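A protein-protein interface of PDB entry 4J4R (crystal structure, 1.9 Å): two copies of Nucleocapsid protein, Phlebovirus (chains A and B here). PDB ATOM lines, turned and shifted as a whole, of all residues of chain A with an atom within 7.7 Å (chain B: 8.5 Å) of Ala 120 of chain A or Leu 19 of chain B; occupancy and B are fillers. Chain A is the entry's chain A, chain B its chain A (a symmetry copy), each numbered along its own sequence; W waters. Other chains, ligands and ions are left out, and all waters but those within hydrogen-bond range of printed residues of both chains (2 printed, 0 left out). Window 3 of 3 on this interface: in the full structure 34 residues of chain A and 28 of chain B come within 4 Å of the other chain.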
ATOM      1  N   LYS A  58      -5.277  30.259  14.770  1.00  0.00           N
ATOM      2  CA  LYS A  58      -5.414  29.683  16.110  1.00  0.00           C
ATOM      3  C   LYS A  58      -5.119  30.716  17.189  1.00  0.00           C
ATOM      4  O   LYS A  58      -5.841  30.798  18.179  1.00  0.00           O
ATOM      5  CB  LYS A  58      -4.541  28.421  16.254  1.00  0.00           C
ATOM      6  CG  LYS A  58      -5.061  27.241  15.409  1.00  0.00           C
ATOM      7  CD  LYS A  58      -4.163  25.992  15.542  1.00  0.00           C
ATOM      8  CE  LYS A  58      -4.629  24.880  14.588  1.00  0.00           C
ATOM      9  NZ  LYS A  58      -3.675  23.709  14.568  1.00  0.00           N
ATOM     10  N   LEU A  65     -11.435  34.195  22.262  1.00  0.00           N
ATOM     11  CA  LEU A  65     -12.020  33.377  23.326  1.00  0.00           C
ATOM     12  C   LEU A  65     -11.805  34.013  24.691  1.00  0.00           C
ATOM     13  O   LEU A  65     -12.670  33.956  25.566  1.00  0.00           O
ATOM     14  CB  LEU A  65     -11.364  31.992  23.340  1.00  0.00           C
ATOM     15  CG  LEU A  65     -11.917  30.995  22.336  1.00  0.00           C
ATOM     16  CD1 LEU A  65     -11.165  29.673  22.421  1.00  0.00           C
ATOM     17  CD2 LEU A  65     -13.399  30.797  22.628  1.00  0.00           C
ATOM     18  N   LEU A 114     -14.894  28.874  12.475  1.00  0.00           N
ATOM     19  CA  LEU A 114     -14.265  27.578  12.684  1.00  0.00           C
ATOM     20  C   LEU A 114     -14.807  26.975  13.985  1.00  0.00           C
ATOM     21  O   LEU A 114     -14.054  26.747  14.927  1.00  0.00           O
ATOM     22  CB  LEU A 114     -12.747  27.746  12.766  1.00  0.00           C
ATOM     23  CG  LEU A 114     -11.897  28.142  11.545  1.00  0.00           C
ATOM     24  CD1 LEU A 114     -12.354  29.364  10.799  1.00  0.00           C
ATOM     25  CD2 LEU A 114     -10.513  28.422  12.005  1.00  0.00           C
ATOM     26  N   PRO A 115     -16.122  26.702  14.038  1.00  0.00           N
ATOM     27  CA  PRO A 115     -16.714  26.565  15.377  1.00  0.00           C
ATOM     28  C   PRO A 115     -16.317  25.301  16.139  1.00  0.00           C
ATOM     29  O   PRO A 115     -16.248  25.354  17.371  1.00  0.00           O
ATOM     30  CB  PRO A 115     -18.230  26.597  15.098  1.00  0.00           C
ATOM     31  CG  PRO A 115     -18.360  26.106  13.659  1.00  0.00           C
ATOM     32  CD  PRO A 115     -17.132  26.627  12.959  1.00  0.00           C
ATOM     33  N   THR A 116     -16.082  24.186  15.455  1.00  0.00           N
ATOM     34  CA  THR A 116     -15.686  22.973  16.170  1.00  0.00           C
ATOM     35  C   THR A 116     -14.307  23.136  16.800  1.00  0.00           C
ATOM     36  O   THR A 116     -14.058  22.625  17.900  1.00  0.00           O
ATOM     37  CB  THR A 116     -15.730  21.699  15.295  1.00  0.00           C
ATOM     38  OG1 THR A 116     -15.143  21.962  14.009  1.00  0.00           O
ATOM     39  CG2 THR A 116     -17.164  21.215  15.109  1.00  0.00           C
ATOM     40  N   TRP A 117     -13.399  23.828  16.107  1.00  0.00           N
ATOM     41  CA  TRP A 117     -12.079  24.092  16.687  1.00  0.00           C
ATOM     42  C   TRP A 117     -12.205  25.033  17.873  1.00  0.00           C
ATOM     43  O   TRP A 117     -11.638  24.799  18.964  1.00  0.00           O
ATOM     44  CB  TRP A 117     -11.091  24.696  15.668  1.00  0.00           C
ATOM     45  CG  TRP A 117      -9.664  24.606  16.200  1.00  0.00           C
ATOM     46  CD1 TRP A 117      -8.799  23.566  16.037  1.00  0.00           C
ATOM     47  CD2 TRP A 117      -8.979  25.575  17.018  1.00  0.00           C
ATOM     48  NE1 TRP A 117      -7.615  23.827  16.696  1.00  0.00           N
ATOM     49  CE2 TRP A 117      -7.698  25.050  17.304  1.00  0.00           C
ATOM     50  CE3 TRP A 117      -9.323  26.836  17.535  1.00  0.00           C
ATOM     51  CZ2 TRP A 117      -6.756  25.738  18.085  1.00  0.00           C
ATOM     52  CZ3 TRP A 117      -8.386  27.521  18.304  1.00  0.00           C
ATOM     53  CH2 TRP A 117      -7.111  26.968  18.569  1.00  0.00           C
ATOM     54  N   THR A 118     -12.939  26.119  17.661  1.00  0.00           N
ATOM     55  CA  THR A 118     -13.094  27.137  18.686  1.00  0.00           C
ATOM     56  C   THR A 118     -13.680  26.578  19.978  1.00  0.00           C
ATOM     57  O   THR A 118     -13.192  26.887  21.056  1.00  0.00           O
ATOM     58  CB  THR A 118     -13.981  28.278  18.180  1.00  0.00           C
ATOM     59  OG1 THR A 118     -13.298  28.926  17.095  1.00  0.00           O
ATOM     60  CG2 THR A 118     -14.281  29.276  19.311  1.00  0.00           C
ATOM     61  N   CYS A 119     -14.724  25.764  19.875  1.00  0.00           N
ATOM     62  CA  CYS A 119     -15.384  25.253  21.078  1.00  0.00           C
ATOM     63  C   CYS A 119     -14.543  24.203  21.808  1.00  0.00           C
ATOM     64  O   CYS A 119     -14.586  24.123  23.043  1.00  0.00           O
ATOM     65  CB  CYS A 119     -16.785  24.722  20.759  1.00  0.00           C
ATOM     66  SG  CYS A 119     -17.967  25.986  20.212  1.00  0.00           S
ATOM     67  N   ALA A 120     -13.777  23.405  21.062  1.00  0.00           N
ATOM     68  CA  ALA A 120     -12.803  22.490  21.672  1.00  0.00           C
ATOM     69  C   ALA A 120     -11.698  23.287  22.371  1.00  0.00           C
ATOM     70  O   ALA A 120     -11.247  22.936  23.462  1.00  0.00           O
ATOM     71  CB  ALA A 120     -12.198  21.555  20.634  1.00  0.00           C
ATOM     72  N   ALA A 121     -11.260  24.371  21.747  1.00  0.00           N
ATOM     73  CA  ALA A 121     -10.240  25.216  22.348  1.00  0.00           C
ATOM     74  C   ALA A 121     -10.771  25.913  23.603  1.00  0.00           C
ATOM     75  O   ALA A 121     -10.055  26.052  24.599  1.00  0.00           O
ATOM     76  CB  ALA A 121      -9.716  26.232  21.335  1.00  0.00           C
ATOM     77  N   ALA A 122     -12.017  26.372  23.549  1.00  0.00           N
ATOM     78  CA  ALA A 122     -12.653  26.972  24.723  1.00  0.00           C
ATOM     79  C   ALA A 122     -12.671  25.997  25.907  1.00  0.00           C
ATOM     80  O   ALA A 122     -12.326  26.365  27.041  1.00  0.00           O
ATOM     81  CB  ALA A 122     -14.058  27.431  24.389  1.00  0.00           C
ATOM     82  N   ALA A 123     -13.054  24.748  25.652  1.00  0.00           N
ATOM     83  CA  ALA A 123     -13.077  23.770  26.738  1.00  0.00           C
ATOM     84  C   ALA A 123     -11.665  23.552  27.296  1.00  0.00           C
ATOM     85  O   ALA A 123     -11.468  23.525  28.522  1.00  0.00           O
ATOM     86  CB  ALA A 123     -13.716  22.455  26.288  1.00  0.00           C
ATOM     87  N   ALA A 124     -10.686  23.442  26.400  1.00  0.00           N
ATOM     88  CA  ALA A 124      -9.288  23.249  26.789  1.00  0.00           C
ATOM     89  C   ALA A 124      -8.759  24.417  27.607  1.00  0.00           C
ATOM     90  O   ALA A 124      -7.966  24.227  28.529  1.00  0.00           O
ATOM     91  CB  ALA A 124      -8.420  23.047  25.566  1.00  0.00           C
ATOM     92  N   LEU A 125      -9.199  25.623  27.259  1.00  0.00           N
ATOM     93  CA  LEU A 125      -8.731  26.833  27.920  1.00  0.00           C
ATOM     94  C   LEU A 125      -9.761  27.396  28.889  1.00  0.00           C
ATOM     95  O   LEU A 125      -9.769  28.601  29.153  1.00  0.00           O
ATOM     96  CB  LEU A 125      -8.351  27.893  26.875  1.00  0.00           C
ATOM     97  CG  LEU A 125      -7.219  27.503  25.926  1.00  0.00           C
ATOM     98  CD1 LEU A 125      -7.004  28.567  24.847  1.00  0.00           C
ATOM     99  CD2 LEU A 125      -5.928  27.250  26.666  1.00  0.00           C
ATOM    100  N   LYS A 126     -10.626  26.539  29.436  1.00  0.00           N
ATOM    101  CA  LYS A 126     -11.761  27.044  30.222  1.00  0.00           C
ATOM    102  C   LYS A 126     -11.354  27.906  31.441  1.00  0.00           C
ATOM    103  O   LYS A 126     -12.071  28.844  31.821  1.00  0.00           O
ATOM    104  CB  LYS A 126     -12.697  25.895  30.633  1.00  0.00           C
ATOM    105  CG  LYS A 126     -12.108  24.943  31.657  1.00  0.00           C
ATOM    106  CD  LYS A 126     -13.058  23.763  31.862  1.00  0.00           C
ATOM    107  CE  LYS A 126     -12.546  22.831  32.949  1.00  0.00           C
ATOM    108  NZ  LYS A 126     -13.436  21.639  33.108  1.00  0.00           N
ATOM    109  N   PRO A 145     -18.238  22.745  29.088  1.00  0.00           N
ATOM    110  CA  PRO A 145     -17.273  23.814  28.815  1.00  0.00           C
ATOM    111  C   PRO A 145     -17.244  24.219  27.339  1.00  0.00           C
ATOM    112  O   PRO A 145     -16.818  25.333  27.036  1.00  0.00           O
ATOM    113  CB  PRO A 145     -15.933  23.190  29.233  1.00  0.00           C
ATOM    114  CG  PRO A 145     -16.299  22.109  30.199  1.00  0.00           C
ATOM    115  CD  PRO A 145     -17.608  21.567  29.706  1.00  0.00           C
ATOM    116  N   GLU A 146     -17.679  23.334  26.446  1.00  0.00           N
ATOM    117  CA  GLU A 146     -17.714  23.645  25.012  1.00  0.00           C
ATOM    118  C   GLU A 146     -18.727  24.739  24.672  1.00  0.00           C
ATOM    119  O   GLU A 146     -18.607  25.413  23.630  1.00  0.00           O
ATOM    120  CB  GLU A 146     -18.010  22.389  24.187  1.00  0.00           C
ATOM    121  CG  GLU A 146     -16.878  21.368  24.173  1.00  0.00           C
ATOM    122  CD  GLU A 146     -16.915  20.437  25.374  1.00  0.00           C
ATOM    123  OE1 GLU A 146     -17.872  20.530  26.185  1.00  0.00           O
ATOM    124  OE2 GLU A 146     -15.983  19.614  25.502  1.00  0.00           O
ATOM    125  N   MET A 147     -19.716  24.905  25.552  1.00  0.00           N
ATOM    126  CA  MET A 147     -20.733  25.951  25.422  1.00  0.00           C
ATOM    127  C   MET A 147     -20.283  27.323  25.933  1.00  0.00           C
ATOM    128  O   MET A 147     -21.012  28.308  25.783  1.00  0.00           O
ATOM    129  CB  MET A 147     -22.001  25.555  26.186  1.00  0.00           C
ATOM    130  CG  MET A 147     -22.717  24.331  25.669  1.00  0.00           C
ATOM    131  SD  MET A 147     -24.345  24.173  26.449  1.00  0.00           S
ATOM    132  CE  MET A 147     -24.851  22.605  25.733  1.00  0.00           C
ATOM    133  N   CYS A 149     -18.536  29.768  24.999  1.00  0.00           N
ATOM    134  CA  CYS A 149     -17.921  30.636  24.000  1.00  0.00           C
ATOM    135  C   CYS A 149     -18.919  31.084  22.943  1.00  0.00           C
ATOM    136  O   CYS A 149     -19.999  30.504  22.806  1.00  0.00           O
ATOM    137  CB  CYS A 149     -16.706  29.962  23.351  1.00  0.00           C
ATOM    138  SG  CYS A 149     -17.077  28.680  22.127  1.00  0.00           S
ATOM    139  N   LEU A 155     -23.008  25.097  16.397  1.00  0.00           N
ATOM    140  CA  LEU A 155     -22.918  23.640  16.523  1.00  0.00           C
ATOM    141  C   LEU A 155     -24.230  22.987  16.969  1.00  0.00           C
ATOM    142  O   LEU A 155     -24.307  21.772  17.106  1.00  0.00           O
ATOM    143  CB  LEU A 155     -21.795  23.260  17.485  1.00  0.00           C
ATOM    144  CG  LEU A 155     -20.438  23.830  17.090  1.00  0.00           C
ATOM    145  CD1 LEU A 155     -19.382  23.401  18.085  1.00  0.00           C
ATOM    146  CD2 LEU A 155     -20.069  23.382  15.679  1.00  0.00           C
ATOM    147  N   TRP A 221     -20.178  15.587  16.280  1.00  0.00           N
ATOM    148  CA  TRP A 221     -19.287  16.270  17.215  1.00  0.00           C
ATOM    149  C   TRP A 221     -19.907  16.371  18.615  1.00  0.00           C
ATOM    150  O   TRP A 221     -19.223  16.135  19.611  1.00  0.00           O
ATOM    151  CB  TRP A 221     -18.921  17.655  16.655  1.00  0.00           C
ATOM    152  CG  TRP A 221     -17.846  18.422  17.404  1.00  0.00           C
ATOM    153  CD1 TRP A 221     -16.502  18.434  17.140  1.00  0.00           C
ATOM    154  CD2 TRP A 221     -18.045  19.326  18.500  1.00  0.00           C
ATOM    155  NE1 TRP A 221     -15.856  19.277  18.020  1.00  0.00           N
ATOM    156  CE2 TRP A 221     -16.783  19.838  18.860  1.00  0.00           C
ATOM    157  CE3 TRP A 221     -19.171  19.745  19.217  1.00  0.00           C
ATOM    158  CZ2 TRP A 221     -16.614  20.744  19.913  1.00  0.00           C
ATOM    159  CZ3 TRP A 221     -19.003  20.649  20.262  1.00  0.00           C
ATOM    160  CH2 TRP A 221     -17.734  21.135  20.598  1.00  0.00           C
ATOM    161  N   LYS A 225     -18.497  14.726  22.108  1.00  0.00           N
ATOM    162  CA  LYS A 225     -18.229  15.508  23.310  1.00  0.00           C
ATOM    163  C   LYS A 225     -19.160  15.151  24.463  1.00  0.00           C
ATOM    164  O   LYS A 225     -18.979  15.638  25.580  1.00  0.00           O
ATOM    165  CB  LYS A 225     -18.338  17.014  23.025  1.00  0.00           C
ATOM    166  CG  LYS A 225     -17.366  17.522  21.977  1.00  0.00           C
ATOM    167  CD  LYS A 225     -15.915  17.267  22.356  1.00  0.00           C
ATOM    168  CE  LYS A 225     -14.989  17.675  21.202  1.00  0.00           C
ATOM    169  NZ  LYS A 225     -13.543  17.609  21.591  1.00  0.00           N
ATOM    170  N   PHE B  14     -10.431  21.750   9.792  1.00  0.00           N
ATOM    171  CA  PHE B  14      -9.757  22.574  10.791  1.00  0.00           C
ATOM    172  C   PHE B  14     -10.122  22.066  12.191  1.00  0.00           C
ATOM    173  O   PHE B  14      -9.261  21.948  13.075  1.00  0.00           O
ATOM    174  CB  PHE B  14     -10.189  24.036  10.647  1.00  0.00           C
ATOM    175  CG  PHE B  14      -9.223  25.024  11.257  1.00  0.00           C
ATOM    176  CD1 PHE B  14      -8.378  25.781  10.444  1.00  0.00           C
ATOM    177  CD2 PHE B  14      -9.160  25.201  12.635  1.00  0.00           C
ATOM    178  CE1 PHE B  14      -7.480  26.696  11.002  1.00  0.00           C
ATOM    179  CE2 PHE B  14      -8.272  26.118  13.193  1.00  0.00           C
ATOM    180  CZ  PHE B  14      -7.435  26.864  12.375  1.00  0.00           C
ATOM    181  N   GLY B  15     -11.399  21.760  12.390  1.00  0.00           N
ATOM    182  CA  GLY B  15     -11.881  21.299  13.682  1.00  0.00           C
ATOM    183  C   GLY B  15     -11.600  19.840  13.976  1.00  0.00           C
ATOM    184  O   GLY B  15     -11.866  19.372  15.085  1.00  0.00           O
ATOM    185  N   GLU B  16     -11.072  19.103  13.004  1.00  0.00           N
ATOM    186  CA  GLU B  16     -10.699  17.714  13.271  1.00  0.00           C
ATOM    187  C   GLU B  16      -9.259  17.611  13.773  1.00  0.00           C
ATOM    188  O   GLU B  16      -8.821  16.533  14.176  1.00  0.00           O
ATOM    189  CB  GLU B  16     -10.921  16.825  12.031  1.00  0.00           C
ATOM    190  CG  GLU B  16     -12.387  16.719  11.623  1.00  0.00           C
ATOM    191  CD  GLU B  16     -12.614  15.867  10.383  1.00  0.00           C
ATOM    192  OE1 GLU B  16     -12.202  16.280   9.281  1.00  0.00           O
ATOM    193  OE2 GLU B  16     -13.222  14.784  10.506  1.00  0.00           O
ATOM    194  N   GLN B  17      -8.525  18.726  13.745  1.00  0.00           N
ATOM    195  CA  GLN B  17      -7.138  18.751  14.221  1.00  0.00           C
ATOM    196  C   GLN B  17      -7.084  18.459  15.715  1.00  0.00           C
ATOM    197  O   GLN B  17      -7.983  18.840  16.466  1.00  0.00           O
ATOM    198  CB  GLN B  17      -6.497  20.129  14.002  1.00  0.00           C
ATOM    199  CG  GLN B  17      -6.269  20.558  12.568  1.00  0.00           C
ATOM    200  CD  GLN B  17      -5.720  21.991  12.488  1.00  0.00           C
ATOM    201  OE1 GLN B  17      -4.512  22.206  12.354  1.00  0.00           O
ATOM    202  NE2 GLN B  17      -6.617  22.975  12.600  1.00  0.00           N
ATOM    203  N   GLN B  18      -6.022  17.797  16.158  1.00  0.00           N
ATOM    204  CA  GLN B  18      -5.820  17.622  17.586  1.00  0.00           C
ATOM    205  C   GLN B  18      -5.364  18.954  18.159  1.00  0.00           C
ATOM    206  O   GLN B  18      -4.723  19.733  17.457  1.00  0.00           O
ATOM    207  CB  GLN B  18      -4.772  16.541  17.838  1.00  0.00           C
ATOM    208  CG  GLN B  18      -5.241  15.167  17.393  1.00  0.00           C
ATOM    209  CD  GLN B  18      -6.451  14.698  18.169  1.00  0.00           C
ATOM    210  OE1 GLN B  18      -6.563  14.947  19.373  1.00  0.00           O
ATOM    211  NE2 GLN B  18      -7.374  14.022  17.485  1.00  0.00           N
ATOM    212  N   LEU B  19      -5.696  19.230  19.419  1.00  0.00           N
ATOM    213  CA  LEU B  19      -5.221  20.456  20.057  1.00  0.00           C
ATOM    214  C   LEU B  19      -3.817  20.234  20.578  1.00  0.00           C
ATOM    215  O   LEU B  19      -3.523  19.173  21.135  1.00  0.00           O
ATOM    216  CB  LEU B  19      -6.118  20.833  21.227  1.00  0.00           C
ATOM    217  CG  LEU B  19      -7.589  21.036  20.893  1.00  0.00           C
ATOM    218  CD1 LEU B  19      -8.344  21.463  22.138  1.00  0.00           C
ATOM    219  CD2 LEU B  19      -7.719  22.080  19.802  1.00  0.00           C
ATOM    220  N   ASN B  20      -2.948  21.221  20.381  1.00  0.00           N
ATOM    221  CA  ASN B  20      -1.634  21.223  21.012  1.00  0.00           C
ATOM    222  C   ASN B  20      -1.772  22.029  22.287  1.00  0.00           C
ATOM    223  O   ASN B  20      -1.718  23.257  22.246  1.00  0.00           O
ATOM    224  CB  ASN B  20      -0.615  21.869  20.075  1.00  0.00           C
ATOM    225  CG  ASN B  20       0.808  21.808  20.611  1.00  0.00           C
ATOM    226  OD1 ASN B  20       1.037  21.648  21.819  1.00  0.00           O
ATOM    227  ND2 ASN B  20       1.777  21.943  19.708  1.00  0.00           N
ATOM    228  N   LEU B  21      -1.961  21.344  23.415  1.00  0.00           N
ATOM    229  CA  LEU B  21      -2.302  22.016  24.661  1.00  0.00           C
ATOM    230  C   LEU B  21      -1.182  22.896  25.172  1.00  0.00           C
ATOM    231  O   LEU B  21      -1.433  23.976  25.687  1.00  0.00           O
ATOM    232  CB  LEU B  21      -2.723  21.002  25.735  1.00  0.00           C
ATOM    233  CG  LEU B  21      -3.971  20.180  25.388  1.00  0.00           C
ATOM    234  CD1 LEU B  21      -4.370  19.272  26.550  1.00  0.00           C
ATOM    235  CD2 LEU B  21      -5.140  21.084  24.995  1.00  0.00           C
ATOM    236  N   THR B  22       0.058  22.434  25.032  1.00  0.00           N
ATOM    237  CA  THR B  22       1.211  23.230  25.460  1.00  0.00           C
ATOM    238  C   THR B  22       1.249  24.563  24.718  1.00  0.00           C
ATOM    239  O   THR B  22       1.485  25.625  25.313  1.00  0.00           O
ATOM    240  CB  THR B  22       2.511  22.457  25.198  1.00  0.00           C
ATOM    241  OG1 THR B  22       2.469  21.230  25.940  1.00  0.00           O
ATOM    242  CG2 THR B  22       3.728  23.247  25.623  1.00  0.00           C
ATOM    243  N   GLU B  23       1.017  24.499  23.413  1.00  0.00           N
ATOM    244  CA  GLU B  23       1.029  25.681  22.567  1.00  0.00           C
ATOM    245  C   GLU B  23      -0.178  26.584  22.862  1.00  0.00           C
ATOM    246  O   GLU B  23      -0.036  27.800  22.986  1.00  0.00           O
ATOM    247  CB  GLU B  23       1.054  25.254  21.100  1.00  0.00           C
ATOM    248  CG  GLU B  23       0.810  26.371  20.105  1.00  0.00           C
ATOM    249  CD  GLU B  23       0.968  25.902  18.660  1.00  0.00           C
ATOM    250  OE1 GLU B  23      -0.010  25.388  18.068  1.00  0.00           O
ATOM    251  OE2 GLU B  23       2.077  26.053  18.118  1.00  0.00           O
ATOM    252  N   LEU B  24      -1.358  25.988  23.012  1.00  0.00           N
ATOM    253  CA  LEU B  24      -2.559  26.766  23.343  1.00  0.00           C
ATOM    254  C   LEU B  24      -2.462  27.479  24.699  1.00  0.00           C
ATOM    255  O   LEU B  24      -2.907  28.619  24.830  1.00  0.00           O
ATOM    256  CB  LEU B  24      -3.821  25.895  23.271  1.00  0.00           C
ATOM    257  CG  LEU B  24      -4.294  25.512  21.869  1.00  0.00           C
ATOM    258  CD1 LEU B  24      -5.642  24.807  21.932  1.00  0.00           C
ATOM    259  CD2 LEU B  24      -4.374  26.749  20.974  1.00  0.00           C
HETATM  260  O   HOH W   1     -13.058  20.052  17.536  1.00  0.00           O
HETATM  261  O   HOH W   2      -5.001  22.524  16.643  1.00  0.00           O
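The side-chain amino group (NZ) of Lys 58 of chain A lies within hydrogen-bond range of the side-chain amide oxygen (OE1) of Gln 17 of chain B, 2.8 Å away.
The backbone carbonyl oxygen of Leu 114 of chain A sits at hydrogen-bond distance from the side-chain hydroxyl of Thr 118 of chain A (3.2 Å). The backbone carbonyl oxygen (O) of Phe 14 of chain B is in hydrogen-bond range of the side-chain amide nitrogen (NE2) of Gln 17 of chain B (2.9 Å).
Phe 14 of chain B touches Lys 58 of chain A (CZ to CG, 3.9 Å). Leu 114 of chain A touches Phe 14 of chain B. CA of Gly 15 of chain B touches OG1 of Thr 116 of chain A, 3.3 Å away. Trp 117 of chain A touches Phe 14 of chain B (CD1 to O, 3.4 Å). Gly 15 of chain B touches Trp 117 of chain A. NE1 of Trp 117 of chain A touches CD2 of Leu 19 of chain B, 3.6 Å away. CH2 of Trp 117 of chain A touches CD2 of Leu 24 of chain B (3.7 Å). Leu 19 of chain B touches Ala 120 of chain A (CD1 to O, 3.5 Å). Ala 124 of chain A touches Leu 19 of chain B (CB to CD1, 3.8 Å). CD2 of Leu 125 of chain A touches O of Leu 24 of chain B, at 3.8 Å.
Of the printed residues of chain B, Thr 116 of chain A touches Gly 15. Ala 120 of chain A touches just one residue of chain B: Leu 19 (3.5 Å). Printed residues of chain B within 4 Å of Ala 124 of chain A: Leu 19 (3.8 Å) and Leu 21 (3.9 Å). Cys 149 of chain A touches none of the printed residues of chain B. Of chain A, only Trp 117 (3.6 Å), Ala 120 (3.5 Å) and Ala 124 (3.8 Å) come within 4 Å of Leu 19 of chain B.
Among the printed residues, 12 pairs touch across the chains. Among the printed residues, no Asp or Glu carboxylate lies within 4 Å of a Lys or Arg side-chain nitrogen of the other chain.
No position is printed for both chains.
Water W2 lies within hydrogen-bond range of the side-chain amino group (NZ) of Lys 58 of chain A (2.7 Å), the backbone carbonyl oxygen (O) of Gln 18 of chain B (2.9 Å) and the indole nitrogen (NE1) of Trp 117 of chain A (2.9 Å). Water W1 lies within hydrogen-bond range of O of Thr 116 of chain A (2.8 Å), O of Gly 15 of chain B (2.8 Å) and NE1 of Trp 221 of chain A (2.9 Å).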
